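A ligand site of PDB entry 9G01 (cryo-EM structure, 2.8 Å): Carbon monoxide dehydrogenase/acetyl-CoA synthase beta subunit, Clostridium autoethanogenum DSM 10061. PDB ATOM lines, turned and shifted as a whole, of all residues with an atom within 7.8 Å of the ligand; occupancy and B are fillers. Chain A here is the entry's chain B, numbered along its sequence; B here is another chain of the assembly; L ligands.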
ATOM      1  N   GLN A  36       0.573  -5.167  20.194  1.00  0.00           N
ATOM      2  CA  GLN A  36       1.045  -6.229  21.068  1.00  0.00           C
ATOM      3  C   GLN A  36       0.665  -7.594  20.502  1.00  0.00           C
ATOM      4  O   GLN A  36      -0.298  -7.745  19.740  1.00  0.00           O
ATOM      5  CB  GLN A  36       0.488  -6.016  22.481  1.00  0.00           C
ATOM      6  CG  GLN A  36       1.115  -4.770  23.149  1.00  0.00           C
ATOM      7  CD  GLN A  36       0.540  -4.488  24.538  1.00  0.00           C
ATOM      8  OE1 GLN A  36      -0.644  -4.190  24.674  1.00  0.00           O
ATOM      9  NE2 GLN A  36       1.369  -4.606  25.575  1.00  0.00           N
ATOM     10  N   CYS A  37       1.437  -8.611  20.903  1.00  0.00           N
ATOM     11  CA  CYS A  37       1.279  -9.928  20.307  1.00  0.00           C
ATOM     12  C   CYS A  37      -0.143 -10.462  20.502  1.00  0.00           C
ATOM     13  O   CYS A  37      -0.618 -10.591  21.629  1.00  0.00           O
ATOM     14  CB  CYS A  37       2.287 -10.903  20.904  1.00  0.00           C
ATOM     15  SG  CYS A  37       2.002 -12.623  20.361  1.00  0.00           S
ATOM     16  N   GLY A  38      -0.761 -10.870  19.395  1.00  0.00           N
ATOM     17  CA  GLY A  38      -2.121 -11.377  19.454  1.00  0.00           C
ATOM     18  C   GLY A  38      -2.249 -12.658  20.257  1.00  0.00           C
ATOM     19  O   GLY A  38      -3.204 -12.830  21.002  1.00  0.00           O
ATOM     20  N   PHE A  39      -1.260 -13.562  20.117  1.00  0.00           N
ATOM     21  CA  PHE A  39      -1.307 -14.831  20.853  1.00  0.00           C
ATOM     22  C   PHE A  39      -1.266 -14.596  22.357  1.00  0.00           C
ATOM     23  O   PHE A  39      -2.061 -15.158  23.108  1.00  0.00           O
ATOM     24  CB  PHE A  39      -0.140 -15.739  20.439  1.00  0.00           C
ATOM     25  CG  PHE A  39      -0.173 -16.150  19.002  1.00  0.00           C
ATOM     26  CD1 PHE A  39      -1.084 -17.117  18.563  1.00  0.00           C
ATOM     27  CD2 PHE A  39       0.691 -15.558  18.075  1.00  0.00           C
ATOM     28  CE1 PHE A  39      -1.127 -17.505  17.214  1.00  0.00           C
ATOM     29  CE2 PHE A  39       0.659 -15.925  16.723  1.00  0.00           C
ATOM     30  CZ  PHE A  39      -0.255 -16.905  16.280  1.00  0.00           C
ATOM     31  N   GLY A  40      -0.331 -13.754  22.805  1.00  0.00           N
ATOM     32  CA  GLY A  40      -0.256 -13.433  24.220  1.00  0.00           C
ATOM     33  C   GLY A  40      -1.474 -12.672  24.717  1.00  0.00           C
ATOM     34  O   GLY A  40      -1.923 -12.860  25.851  1.00  0.00           O
ATOM     35  N   SER A  41      -2.009 -11.780  23.878  1.00  0.00           N
ATOM     36  CA  SER A  41      -3.191 -11.017  24.263  1.00  0.00           C
ATOM     37  C   SER A  41      -4.401 -11.939  24.455  1.00  0.00           C
ATOM     38  O   SER A  41      -5.209 -11.717  25.353  1.00  0.00           O
ATOM     39  CB  SER A  41      -3.503  -9.935  23.224  1.00  0.00           C
ATOM     40  OG  SER A  41      -2.412  -9.046  23.059  1.00  0.00           O
ATOM     41  N   ALA A  42      -4.530 -12.975  23.625  1.00  0.00           N
ATOM     42  CA  ALA A  42      -5.629 -13.915  23.765  1.00  0.00           C
ATOM     43  C   ALA A  42      -5.343 -15.025  24.785  1.00  0.00           C
ATOM     44  O   ALA A  42      -6.261 -15.775  25.129  1.00  0.00           O
ATOM     45  CB  ALA A  42      -5.988 -14.539  22.404  1.00  0.00           C
ATOM     46  N   GLY A  43      -4.108 -15.148  25.257  1.00  0.00           N
ATOM     47  CA  GLY A  43      -3.758 -16.171  26.220  1.00  0.00           C
ATOM     48  C   GLY A  43      -3.526 -17.555  25.642  1.00  0.00           C
ATOM     49  O   GLY A  43      -3.498 -18.529  26.397  1.00  0.00           O
ATOM     50  N   VAL A  44      -3.346 -17.665  24.314  1.00  0.00           N
ATOM     51  CA  VAL A  44      -3.154 -18.942  23.639  1.00  0.00           C
ATOM     52  C   VAL A  44      -1.682 -19.270  23.423  1.00  0.00           C
ATOM     53  O   VAL A  44      -1.357 -20.198  22.670  1.00  0.00           O
ATOM     54  CB  VAL A  44      -3.935 -19.013  22.315  1.00  0.00           C
ATOM     55  CG1 VAL A  44      -5.424 -19.251  22.607  1.00  0.00           C
ATOM     56  CG2 VAL A  44      -3.730 -17.740  21.472  1.00  0.00           C
ATOM     57  N   CYS A  45      -0.774 -18.513  24.034  1.00  0.00           N
ATOM     58  CA  CYS A  45       0.650 -18.830  23.995  1.00  0.00           C
ATOM     59  C   CYS A  45       1.037 -19.533  25.283  1.00  0.00           C
ATOM     60  O   CYS A  45       0.595 -19.129  26.367  1.00  0.00           O
ATOM     61  CB  CYS A  45       1.506 -17.570  23.826  1.00  0.00           C
ATOM     62  SG  CYS A  45       3.289 -17.888  24.019  1.00  0.00           S
ATOM     63  N   CYS A  46       1.879 -20.556  25.177  1.00  0.00           N
ATOM     64  CA  CYS A  46       2.331 -21.292  26.335  1.00  0.00           C
ATOM     65  C   CYS A  46       3.847 -21.395  26.325  1.00  0.00           C
ATOM     66  O   CYS A  46       4.466 -21.586  25.284  1.00  0.00           O
ATOM     67  CB  CYS A  46       1.723 -22.706  26.378  1.00  0.00           C
ATOM     68  SG  CYS A  46       2.155 -23.583  27.901  1.00  0.00           S
ATOM     69  N   ARG A  47       4.456 -21.229  27.512  1.00  0.00           N
ATOM     70  CA  ARG A  47       5.897 -21.400  27.658  1.00  0.00           C
ATOM     71  C   ARG A  47       6.221 -22.225  28.890  1.00  0.00           C
ATOM     72  O   ARG A  47       7.315 -22.106  29.452  1.00  0.00           O
ATOM     73  CB  ARG A  47       6.610 -20.045  27.717  1.00  0.00           C
ATOM     74  CG  ARG A  47       6.438 -19.207  26.432  1.00  0.00           C
ATOM     75  CD  ARG A  47       7.444 -18.039  26.380  1.00  0.00           C
ATOM     76  NE  ARG A  47       7.343 -17.198  27.564  1.00  0.00           N
ATOM     77  CZ  ARG A  47       6.623 -16.085  27.625  1.00  0.00           C
ATOM     78  NH1 ARG A  47       5.987 -15.603  26.579  1.00  0.00           N
ATOM     79  NH2 ARG A  47       6.543 -15.428  28.792  1.00  0.00           N
ATOM     80  N   PRO A  53       8.469 -22.631  22.977  1.00  0.00           N
ATOM     81  CA  PRO A  53       7.112 -22.019  23.118  1.00  0.00           C
ATOM     82  C   PRO A  53       6.081 -22.552  22.137  1.00  0.00           C
ATOM     83  O   PRO A  53       6.400 -22.829  20.988  1.00  0.00           O
ATOM     84  CB  PRO A  53       7.370 -20.510  22.847  1.00  0.00           C
ATOM     85  CG  PRO A  53       8.890 -20.310  22.867  1.00  0.00           C
ATOM     86  CD  PRO A  53       9.457 -21.661  22.467  1.00  0.00           C
ATOM     87  N   CYS A  54       4.820 -22.706  22.585  1.00  0.00           N
ATOM     88  CA  CYS A  54       3.716 -23.162  21.746  1.00  0.00           C
ATOM     89  C   CYS A  54       2.664 -22.063  21.667  1.00  0.00           C
ATOM     90  O   CYS A  54       2.312 -21.449  22.687  1.00  0.00           O
ATOM     91  CB  CYS A  54       3.057 -24.452  22.287  1.00  0.00           C
ATOM     92  SG  CYS A  54       4.098 -25.935  22.284  1.00  0.00           S
ATOM     93  N   ARG A  55       2.178 -21.813  20.461  1.00  0.00           N
ATOM     94  CA  ARG A  55       1.049 -20.931  20.248  1.00  0.00           C
ATOM     95  C   ARG A  55       0.027 -21.682  19.407  1.00  0.00           C
ATOM     96  O   ARG A  55       0.370 -22.305  18.394  1.00  0.00           O
ATOM     97  CB  ARG A  55       1.468 -19.616  19.591  1.00  0.00           C
ATOM     98  CG  ARG A  55       2.439 -19.748  18.454  1.00  0.00           C
ATOM     99  CD  ARG A  55       3.046 -18.385  18.138  1.00  0.00           C
ATOM    100  NE  ARG A  55       3.982 -18.513  17.033  1.00  0.00           N
ATOM    101  CZ  ARG A  55       4.850 -17.583  16.631  1.00  0.00           C
ATOM    102  NH1 ARG A  55       4.940 -16.426  17.255  1.00  0.00           N
ATOM    103  NH2 ARG A  55       5.638 -17.838  15.590  1.00  0.00           N
ATOM    104  N   GLN B  36       9.323 -21.864  16.068  1.00  0.00           N
ATOM    105  CA  GLN B  36       8.759 -21.374  17.316  1.00  0.00           C
ATOM    106  C   GLN B  36       9.147 -19.912  17.546  1.00  0.00           C
ATOM    107  O   GLN B  36      10.160 -19.420  17.034  1.00  0.00           O
ATOM    108  CB  GLN B  36       9.203 -22.261  18.485  1.00  0.00           C
ATOM    109  CG  GLN B  36       8.540 -23.653  18.428  1.00  0.00           C
ATOM    110  CD  GLN B  36       9.047 -24.592  19.534  1.00  0.00           C
ATOM    111  OE1 GLN B  36      10.233 -24.884  19.596  1.00  0.00           O
ATOM    112  NE2 GLN B  36       8.148 -25.043  20.403  1.00  0.00           N
ATOM    113  N   CYS B  37       8.334 -19.219  18.331  1.00  0.00           N
ATOM    114  CA  CYS B  37       8.509 -17.784  18.483  1.00  0.00           C
ATOM    115  C   CYS B  37       9.894 -17.452  19.020  1.00  0.00           C
ATOM    116  O   CYS B  37      10.283 -17.913  20.103  1.00  0.00           O
ATOM    117  CB  CYS B  37       7.427 -17.214  19.411  1.00  0.00           C
ATOM    118  SG  CYS B  37       7.733 -15.456  19.799  1.00  0.00           S
ATOM    119  N   GLY B  38      10.591 -16.555  18.323  1.00  0.00           N
ATOM    120  CA  GLY B  38      11.926 -16.179  18.725  1.00  0.00           C
ATOM    121  C   GLY B  38      11.977 -15.461  20.058  1.00  0.00           C
ATOM    122  O   GLY B  38      12.879 -15.699  20.869  1.00  0.00           O
ATOM    123  N   PHE B  39      10.983 -14.591  20.324  1.00  0.00           N
ATOM    124  CA  PHE B  39      10.957 -13.866  21.594  1.00  0.00           C
ATOM    125  C   PHE B  39      10.819 -14.813  22.775  1.00  0.00           C
ATOM    126  O   PHE B  39      11.559 -14.717  23.762  1.00  0.00           O
ATOM    127  CB  PHE B  39       9.808 -12.841  21.626  1.00  0.00           C
ATOM    128  CG  PHE B  39       9.924 -11.766  20.581  1.00  0.00           C
ATOM    129  CD1 PHE B  39      10.826 -10.717  20.752  1.00  0.00           C
ATOM    130  CD2 PHE B  39       9.128 -11.804  19.442  1.00  0.00           C
ATOM    131  CE1 PHE B  39      10.955  -9.701  19.785  1.00  0.00           C
ATOM    132  CE2 PHE B  39       9.233 -10.800  18.450  1.00  0.00           C
ATOM    133  CZ  PHE B  39      10.151  -9.740  18.625  1.00  0.00           C
ATOM    134  N   GLY B  40       9.870 -15.750  22.684  1.00  0.00           N
ATOM    135  CA  GLY B  40       9.699 -16.718  23.745  1.00  0.00           C
ATOM    136  C   GLY B  40      10.882 -17.665  23.870  1.00  0.00           C
ATOM    137  O   GLY B  40      11.243 -18.076  24.976  1.00  0.00           O
ATOM    138  N   SER B  41      11.503 -18.025  22.742  1.00  0.00           N
ATOM    139  CA  SER B  41      12.668 -18.905  22.791  1.00  0.00           C
ATOM    140  C   SER B  41      13.835 -18.228  23.494  1.00  0.00           C
ATOM    141  O   SER B  41      14.592 -18.889  24.228  1.00  0.00           O
ATOM    142  CB  SER B  41      13.077 -19.332  21.378  1.00  0.00           C
ATOM    143  OG  SER B  41      12.024 -20.007  20.710  1.00  0.00           O
ATOM    144  N   ALA B  42      14.012 -16.913  23.303  1.00  0.00           N
ATOM    145  CA  ALA B  42      15.079 -16.190  23.974  1.00  0.00           C
ATOM    146  C   ALA B  42      14.697 -15.727  25.377  1.00  0.00           C
ATOM    147  O   ALA B  42      15.579 -15.276  26.123  1.00  0.00           O
ATOM    148  CB  ALA B  42      15.525 -14.978  23.134  1.00  0.00           C
ATOM    149  N   GLY B  43      13.429 -15.833  25.765  1.00  0.00           N
ATOM    150  CA  GLY B  43      12.983 -15.412  27.082  1.00  0.00           C
ATOM    151  C   GLY B  43      12.773 -13.927  27.253  1.00  0.00           C
ATOM    152  O   GLY B  43      12.678 -13.452  28.391  1.00  0.00           O
ATOM    153  N   VAL B  44      12.674 -13.167  26.157  1.00  0.00           N
ATOM    154  CA  VAL B  44      12.516 -11.712  26.188  1.00  0.00           C
ATOM    155  C   VAL B  44      11.049 -11.296  26.054  1.00  0.00           C
ATOM    156  O   VAL B  44      10.763 -10.108  25.832  1.00  0.00           O
ATOM    157  CB  VAL B  44      13.396 -11.017  25.144  1.00  0.00           C
ATOM    158  CG1 VAL B  44      14.849 -10.977  25.626  1.00  0.00           C
ATOM    159  CG2 VAL B  44      13.279 -11.695  23.757  1.00  0.00           C
ATOM    160  N   CYS B  45      10.114 -12.240  26.138  1.00  0.00           N
ATOM    161  CA  CYS B  45       8.696 -11.925  26.156  1.00  0.00           C
ATOM    162  C   CYS B  45       8.202 -11.950  27.591  1.00  0.00           C
ATOM    163  O   CYS B  45       8.573 -12.835  28.363  1.00  0.00           O
ATOM    164  CB  CYS B  45       7.880 -12.917  25.320  1.00  0.00           C
ATOM    165  SG  CYS B  45       6.076 -12.694  25.516  1.00  0.00           S
ATOM    166  N   CYS B  46       7.359 -10.988  27.949  1.00  0.00           N
ATOM    167  CA  CYS B  46       6.800 -10.923  29.281  1.00  0.00           C
ATOM    168  C   CYS B  46       5.279 -10.808  29.220  1.00  0.00           C
ATOM    169  O   CYS B  46       4.743 -10.103  28.362  1.00  0.00           O
ATOM    170  CB  CYS B  46       7.370  -9.723  30.069  1.00  0.00           C
ATOM    171  SG  CYS B  46       6.830  -9.722  31.788  1.00  0.00           S
ATOM    172  N   ARG B  47       4.597 -11.522  30.111  1.00  0.00           N
ATOM    173  CA  ARG B  47       3.146 -11.419  30.216  1.00  0.00           C
ATOM    174  C   ARG B  47       2.715 -11.313  31.678  1.00  0.00           C
ATOM    175  O   ARG B  47       1.580 -11.664  32.016  1.00  0.00           O
ATOM    176  CB  ARG B  47       2.456 -12.608  29.540  1.00  0.00           C
ATOM    177  CG  ARG B  47       2.747 -12.695  28.036  1.00  0.00           C
ATOM    178  CD  ARG B  47       1.765 -13.652  27.328  1.00  0.00           C
ATOM    179  NE  ARG B  47       1.801 -14.981  27.937  1.00  0.00           N
ATOM    180  CZ  ARG B  47       2.535 -15.995  27.509  1.00  0.00           C
ATOM    181  NH1 ARG B  47       3.264 -15.899  26.413  1.00  0.00           N
ATOM    182  NH2 ARG B  47       2.537 -17.140  28.198  1.00  0.00           N
ATOM    183  N   PRO B  53       0.908  -7.966  26.607  1.00  0.00           N
ATOM    184  CA  PRO B  53       2.255  -8.597  26.512  1.00  0.00           C
ATOM    185  C   PRO B  53       3.353  -7.661  26.007  1.00  0.00           C
ATOM    186  O   PRO B  53       3.113  -6.845  25.139  1.00  0.00           O
ATOM    187  CB  PRO B  53       2.042  -9.758  25.510  1.00  0.00           C
ATOM    188  CG  PRO B  53       0.531  -9.895  25.310  1.00  0.00           C
ATOM    189  CD  PRO B  53      -0.032  -8.515  25.604  1.00  0.00           C
ATOM    190  N   CYS B  54       4.560  -7.776  26.573  1.00  0.00           N
ATOM    191  CA  CYS B  54       5.720  -6.992  26.155  1.00  0.00           C
ATOM    192  C   CYS B  54       6.790  -7.918  25.618  1.00  0.00           C
ATOM    193  O   CYS B  54       7.078  -8.966  26.220  1.00  0.00           O
ATOM    194  CB  CYS B  54       6.312  -6.154  27.304  1.00  0.00           C
ATOM    195  SG  CYS B  54       5.245  -4.846  27.963  1.00  0.00           S
ATOM    196  N   ARG B  55       7.360  -7.550  24.486  1.00  0.00           N
ATOM    197  CA  ARG B  55       8.519  -8.228  23.936  1.00  0.00           C
ATOM    198  C   ARG B  55       9.585  -7.178  23.658  1.00  0.00           C
ATOM    199  O   ARG B  55       9.311  -6.135  23.066  1.00  0.00           O
ATOM    200  CB  ARG B  55       8.175  -9.035  22.692  1.00  0.00           C
ATOM    201  CG  ARG B  55       7.287  -8.336  21.704  1.00  0.00           C
ATOM    202  CD  ARG B  55       6.732  -9.348  20.708  1.00  0.00           C
ATOM    203  NE  ARG B  55       5.863  -8.669  19.757  1.00  0.00           N
ATOM    204  CZ  ARG B  55       5.051  -9.268  18.892  1.00  0.00           C
ATOM    205  NH1 ARG B  55       4.953 -10.578  18.828  1.00  0.00           N
ATOM    206  NH2 ARG B  55       4.308  -8.514  18.080  1.00  0.00           N
HETATM  207 FE1  LIG L   1       3.584 -13.826  21.490  1.00  0.00          FE
HETATM  208 FE2  LIG L   1       5.327 -13.696  23.593  1.00  0.00          FE
HETATM  209 FE3  LIG L   1       6.068 -14.962  21.285  1.00  0.00          FE
HETATM  210 FE4  LIG L   1       4.177 -16.086  22.909  1.00  0.00          FE
HETATM  211  S1  LIG L   1       6.377 -15.716  23.405  1.00  0.00           S
HETATM  212  S2  LIG L   1       4.081 -15.890  20.647  1.00  0.00           S
HETATM  213  S3  LIG L   1       3.105 -14.221  23.676  1.00  0.00           S
HETATM  214  S4  LIG L   1       5.594 -12.739  21.539  1.00  0.00           S
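SG of Cys 37 of chain A binds FE1 of the ligand (2.3 Å).
FE2 of the ligand is bound by SG of Cys 45 of chain B, 2.3 Å away.
NH1 of Arg 55 of chain A lies close to S2 of the ligand (3.5 Å).
SG of Cys 37 of chain B binds FE3 of the ligand, at 2.3 Å.
S4 of the ligand sits close to NH1 of Arg 55 of chain B (3.5 Å).
The backbone NH of Gly 40 of chain B lies close to a sulfur (S1) of the ligand.
The backbone NH (N) of Gly 40 of chain A sits close to a sulfur (S3) of the ligand, at 3.6 Å.
S3 of the ligand sits close to NH1 of Arg 47 of chain B (3.2 Å).
NH1 of Arg 47 of chain A sits close to S1 of the ligand (3.2 Å).
FE4 of the ligand is bound by SG of Cys 45 of chain A.
The backbone carbonyl oxygen (O) of Cys 45 of chain A is in hydrogen-bond range of the guanidinium group (NH2) of Arg 47 of chain B (3.3 Å).
O of Cys 37 of chain A lies within hydrogen-bond range of OG of Ser 41 of chain A (2.8 Å).
N of Gly 40 of chain A sits close to SG of Cys 37 of chain A (3.6 Å).
NH1 of Arg 47 of chain A lies close to NH1 of Arg 47 of chain B.
O of Cys 45 of chain B sits at hydrogen-bond distance from NH2 of Arg 47 of chain A (3.3 Å).
SG of Cys 37 of chain B lies close to N of Phe 39 of chain B, at 3.4 Å.
O of Cys 37 of chain B sits at hydrogen-bond distance from OG of Ser 41 of chain B, 2.8 Å away.
The backbone NH (N) of Phe 39 of chain A lies close to the side-chain sulfur (SG) of Cys 37 of chain A (3.4 Å).
Within 4 Å of the ligand: Cys 37 of chain A, Gly 40 of chain A, Cys 45 of chain A, Arg 47 of chain A, Arg 55 of chain A, Cys 37 of chain B, Gly 40 of chain B, Cys 45 of chain B, Arg 47 of chain B and Arg 55 of chain B.
The nearest printed residue that does not touch the ligand is Phe 39 of chain B (4.2 Å).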
